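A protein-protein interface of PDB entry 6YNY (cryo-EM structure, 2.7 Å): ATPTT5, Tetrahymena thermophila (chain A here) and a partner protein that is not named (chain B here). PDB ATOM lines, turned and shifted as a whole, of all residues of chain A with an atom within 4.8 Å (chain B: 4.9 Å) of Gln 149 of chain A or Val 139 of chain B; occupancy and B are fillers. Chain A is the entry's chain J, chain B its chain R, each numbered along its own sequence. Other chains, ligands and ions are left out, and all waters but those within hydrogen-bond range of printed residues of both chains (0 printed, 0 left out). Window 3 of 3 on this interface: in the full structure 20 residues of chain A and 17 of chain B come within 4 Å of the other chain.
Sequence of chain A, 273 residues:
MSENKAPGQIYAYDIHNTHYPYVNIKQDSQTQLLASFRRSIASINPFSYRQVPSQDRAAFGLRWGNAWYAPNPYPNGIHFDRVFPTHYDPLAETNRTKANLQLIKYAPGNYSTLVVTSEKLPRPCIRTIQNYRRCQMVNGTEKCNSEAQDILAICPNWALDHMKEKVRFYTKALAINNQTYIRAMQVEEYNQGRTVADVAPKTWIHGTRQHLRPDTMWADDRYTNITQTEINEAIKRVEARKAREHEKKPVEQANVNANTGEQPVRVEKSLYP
NZ of Lys 141 of chain B lies within hydrogen-bond range of O of Leu 152 of chain A, 2.7 Å away.
OD1 of Asn 136 of chain B lies close to N of Glu 138 of chain B, 3.5 Å away.
Among the printed residues, pairs that only touch across the chains: Gln 149 of chain A with Val 139 of chain B (3.9 Å), Leu 152 of chain A with Asn 136 of chain B (3.4 Å), Leu 152 of chain A with Val 139 of chain B (3.9 Å), Ala 153 of chain A with Arg 140 of chain B (3.2 Å) and Ala 153 of chain A with Lys 141 of chain B (3.4 Å).
Gln 149 of chain A touches just one residue of chain B: Val 139 (3.9 Å). Ile 151 of chain A touches none of the printed residues of chain B. Of the printed residues of chain B, Leu 152 of chain A touches Asn 136, Val 139 and Lys 141. Of the printed residues of chain A, Asn 136 of chain B touches Leu 152. Val 139 of chain B touches two residues of chain A. Printed residues of chain A within 4 Å of Arg 140 of chain B: Ala 153.
Of the 9 printed residues of chain A, 3 touch a printed residue of chain B. Of the 6 printed residues of chain B, 4 touch a printed residue of chain A. Printed residues of chain B that touch a printed residue of chain A: Asn 136, Val 139, Arg 140 and Lys 141. Hydrophobic or aromatic side chains of chain B within 4 Å of the printed part of chain A: Val 139. Among the printed residues, 6 pairs touch across the chains. Among the printed residues, no Asp or Glu carboxylate lies within 4 Å of a Lys or Arg side-chain nitrogen of the other chain.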
ATOM      1  N   ASN A 145      16.508 -15.197  12.196  1.00  0.00           N
ATOM      2  CA  ASN A 145      17.052 -14.573  13.396  1.00  0.00           C
ATOM      3  C   ASN A 145      16.119 -13.494  13.928  1.00  0.00           C
ATOM      4  O   ASN A 145      15.893 -13.402  15.139  1.00  0.00           O
ATOM      5  CB  ASN A 145      18.431 -13.989  13.102  1.00  0.00           C
ATOM      6  CG  ASN A 145      19.370 -15.003  12.488  1.00  0.00           C
ATOM      7  OD1 ASN A 145      20.061 -15.736  13.194  1.00  0.00           O
ATOM      8  ND2 ASN A 145      19.399 -15.051  11.162  1.00  0.00           N
ATOM      9  N   SER A 146      15.571 -12.666  13.039  1.00  0.00           N
ATOM     10  CA  SER A 146      14.657 -11.618  13.476  1.00  0.00           C
ATOM     11  C   SER A 146      13.407 -12.210  14.111  1.00  0.00           C
ATOM     12  O   SER A 146      12.882 -11.668  15.090  1.00  0.00           O
ATOM     13  CB  SER A 146      14.286 -10.727  12.294  1.00  0.00           C
ATOM     14  OG  SER A 146      13.351  -9.736  12.678  1.00  0.00           O
ATOM     15  N   GLU A 147      12.918 -13.324  13.567  1.00  0.00           N
ATOM     16  CA  GLU A 147      11.740 -13.968  14.131  1.00  0.00           C
ATOM     17  C   GLU A 147      12.058 -14.662  15.446  1.00  0.00           C
ATOM     18  O   GLU A 147      11.166 -14.845  16.280  1.00  0.00           O
ATOM     19  CB  GLU A 147      11.164 -14.966  13.131  1.00  0.00           C
ATOM     20  CG  GLU A 147      10.509 -14.338  11.917  1.00  0.00           C
ATOM     21  CD  GLU A 147      11.502 -13.674  10.988  1.00  0.00           C
ATOM     22  OE1 GLU A 147      12.719 -13.788  11.239  1.00  0.00           O
ATOM     23  OE2 GLU A 147      11.065 -13.034  10.009  1.00  0.00           O
ATOM     24  N   ALA A 148      13.313 -15.063  15.643  1.00  0.00           N
ATOM     25  CA  ALA A 148      13.706 -15.689  16.898  1.00  0.00           C
ATOM     26  C   ALA A 148      13.859 -14.660  18.007  1.00  0.00           C
ATOM     27  O   ALA A 148      13.525 -14.935  19.164  1.00  0.00           O
ATOM     28  CB  ALA A 148      15.007 -16.461  16.711  1.00  0.00           C
ATOM     29  N   GLN A 149      14.367 -13.473  17.676  1.00  0.00           N
ATOM     30  CA  GLN A 149      14.517 -12.431  18.682  1.00  0.00           C
ATOM     31  C   GLN A 149      13.169 -11.882  19.119  1.00  0.00           C
ATOM     32  O   GLN A 149      13.006 -11.498  20.282  1.00  0.00           O
ATOM     33  CB  GLN A 149      15.400 -11.310  18.140  1.00  0.00           C
ATOM     34  CG  GLN A 149      16.825 -11.737  17.850  1.00  0.00           C
ATOM     35  CD  GLN A 149      17.569 -12.170  19.093  1.00  0.00           C
ATOM     36  OE1 GLN A 149      17.785 -11.378  20.008  1.00  0.00           O
ATOM     37  NE2 GLN A 149      17.962 -13.436  19.136  1.00  0.00           N
ATOM     38  N   ASP A 150      12.194 -11.835  18.210  1.00  0.00           N
ATOM     39  CA  ASP A 150      10.856 -11.403  18.591  1.00  0.00           C
ATOM     40  C   ASP A 150      10.244 -12.340  19.619  1.00  0.00           C
ATOM     41  O   ASP A 150       9.490 -11.899  20.492  1.00  0.00           O
ATOM     42  CB  ASP A 150       9.964 -11.319  17.358  1.00  0.00           C
ATOM     43  CG  ASP A 150      10.448 -10.296  16.356  1.00  0.00           C
ATOM     44  OD1 ASP A 150      11.122  -9.330  16.770  1.00  0.00           O
ATOM     45  OD2 ASP A 150      10.153 -10.452  15.153  1.00  0.00           O
ATOM     46  N   ILE A 151      10.558 -13.632  19.535  1.00  0.00           N
ATOM     47  CA  ILE A 151      10.061 -14.584  20.519  1.00  0.00           C
ATOM     48  C   ILE A 151      10.655 -14.289  21.887  1.00  0.00           C
ATOM     49  O   ILE A 151       9.934 -14.168  22.883  1.00  0.00           O
ATOM     50  CB  ILE A 151      10.370 -16.023  20.068  1.00  0.00           C
ATOM     51  CG1 ILE A 151       9.560 -16.359  18.820  1.00  0.00           C
ATOM     52  CG2 ILE A 151      10.083 -17.013  21.184  1.00  0.00           C
ATOM     53  CD1 ILE A 151       9.868 -17.703  18.230  1.00  0.00           C
ATOM     54  N   LEU A 152      11.979 -14.161  21.956  1.00  0.00           N
ATOM     55  CA  LEU A 152      12.636 -13.923  23.232  1.00  0.00           C
ATOM     56  C   LEU A 152      12.238 -12.591  23.848  1.00  0.00           C
ATOM     57  O   LEU A 152      12.367 -12.423  25.065  1.00  0.00           O
ATOM     58  CB  LEU A 152      14.147 -13.978  23.049  1.00  0.00           C
ATOM     59  CG  LEU A 152      14.708 -15.336  22.641  1.00  0.00           C
ATOM     60  CD1 LEU A 152      16.151 -15.210  22.216  1.00  0.00           C
ATOM     61  CD2 LEU A 152      14.578 -16.310  23.783  1.00  0.00           C
ATOM     62  N   ALA A 153      11.756 -11.648  23.046  1.00  0.00           N
ATOM     63  CA  ALA A 153      11.415 -10.318  23.526  1.00  0.00           C
ATOM     64  C   ALA A 153       9.935 -10.150  23.829  1.00  0.00           C
ATOM     65  O   ALA A 153       9.582  -9.573  24.861  1.00  0.00           O
ATOM     66  CB  ALA A 153      11.838  -9.269  22.499  1.00  0.00           C
ATOM     67  N   ASN B 136      21.206 -15.421  28.340  1.00  0.00           N
ATOM     68  CA  ASN B 136      21.025 -14.536  27.192  1.00  0.00           C
ATOM     69  C   ASN B 136      20.862 -13.125  27.740  1.00  0.00           C
ATOM     70  O   ASN B 136      19.778 -12.733  28.174  1.00  0.00           O
ATOM     71  CB  ASN B 136      19.822 -14.964  26.362  1.00  0.00           C
ATOM     72  CG  ASN B 136      19.825 -14.358  24.981  1.00  0.00           C
ATOM     73  OD1 ASN B 136      20.525 -13.381  24.718  1.00  0.00           O
ATOM     74  ND2 ASN B 136      19.037 -14.933  24.085  1.00  0.00           N
ATOM     75  N   VAL B 137      21.952 -12.361  27.722  1.00  0.00           N
ATOM     76  CA  VAL B 137      21.994 -11.037  28.326  1.00  0.00           C
ATOM     77  C   VAL B 137      21.755  -9.932  27.306  1.00  0.00           C
ATOM     78  O   VAL B 137      21.871  -8.750  27.640  1.00  0.00           O
ATOM     79  CB  VAL B 137      23.333 -10.819  29.045  1.00  0.00           C
ATOM     80  CG1 VAL B 137      23.587 -11.936  30.022  1.00  0.00           C
ATOM     81  CG2 VAL B 137      24.463 -10.736  28.039  1.00  0.00           C
ATOM     82  N   GLU B 138      21.413 -10.286  26.071  1.00  0.00           N
ATOM     83  CA  GLU B 138      21.335  -9.325  24.985  1.00  0.00           C
ATOM     84  C   GLU B 138      19.913  -9.012  24.546  1.00  0.00           C
ATOM     85  O   GLU B 138      19.723  -8.094  23.741  1.00  0.00           O
ATOM     86  CB  GLU B 138      22.126  -9.848  23.778  1.00  0.00           C
ATOM     87  CG  GLU B 138      23.553 -10.239  24.106  1.00  0.00           C
ATOM     88  CD  GLU B 138      24.248 -10.931  22.953  1.00  0.00           C
ATOM     89  OE1 GLU B 138      23.586 -11.188  21.927  1.00  0.00           O
ATOM     90  OE2 GLU B 138      25.458 -11.220  23.075  1.00  0.00           O
ATOM     91  N   VAL B 139      18.924  -9.731  25.042  1.00  0.00           N
ATOM     92  CA  VAL B 139      17.545  -9.555  24.606  1.00  0.00           C
ATOM     93  C   VAL B 139      16.852  -8.568  25.529  1.00  0.00           C
ATOM     94  O   VAL B 139      17.061  -8.575  26.748  1.00  0.00           O
ATOM     95  CB  VAL B 139      16.802 -10.902  24.575  1.00  0.00           C
ATOM     96  CG1 VAL B 139      17.613 -11.934  23.825  1.00  0.00           C
ATOM     97  CG2 VAL B 139      16.497 -11.369  25.970  1.00  0.00           C
ATOM     98  N   ARG B 140      16.018  -7.719  24.943  1.00  0.00           N
ATOM     99  CA  ARG B 140      15.267  -6.710  25.671  1.00  0.00           C
ATOM    100  C   ARG B 140      13.785  -7.006  25.527  1.00  0.00           C
ATOM    101  O   ARG B 140      13.279  -7.127  24.406  1.00  0.00           O
ATOM    102  CB  ARG B 140      15.578  -5.309  25.151  1.00  0.00           C
ATOM    103  CG  ARG B 140      17.020  -4.902  25.290  1.00  0.00           C
ATOM    104  CD  ARG B 140      17.203  -3.442  24.960  1.00  0.00           C
ATOM    105  NE  ARG B 140      16.954  -3.157  23.554  1.00  0.00           N
ATOM    106  CZ  ARG B 140      16.650  -1.954  23.081  1.00  0.00           C
ATOM    107  NH1 ARG B 140      16.540  -0.923  23.902  1.00  0.00           N
ATOM    108  NH2 ARG B 140      16.443  -1.786  21.783  1.00  0.00           N
ATOM    109  N   LYS B 141      13.098  -7.124  26.656  1.00  0.00           N
ATOM    110  CA  LYS B 141      11.672  -7.399  26.629  1.00  0.00           C
ATOM    111  C   LYS B 141      10.917  -6.193  26.093  1.00  0.00           C
ATOM    112  O   LYS B 141      11.194  -5.052  26.467  1.00  0.00           O
ATOM    113  CB  LYS B 141      11.170  -7.749  28.028  1.00  0.00           C
ATOM    114  CG  LYS B 141      11.996  -8.785  28.765  1.00  0.00           C
ATOM    115  CD  LYS B 141      12.096 -10.098  28.019  1.00  0.00           C
ATOM    116  CE  LYS B 141      10.757 -10.768  27.869  1.00  0.00           C
ATOM    117  NZ  LYS B 141      10.907 -12.142  27.347  1.00  0.00           N
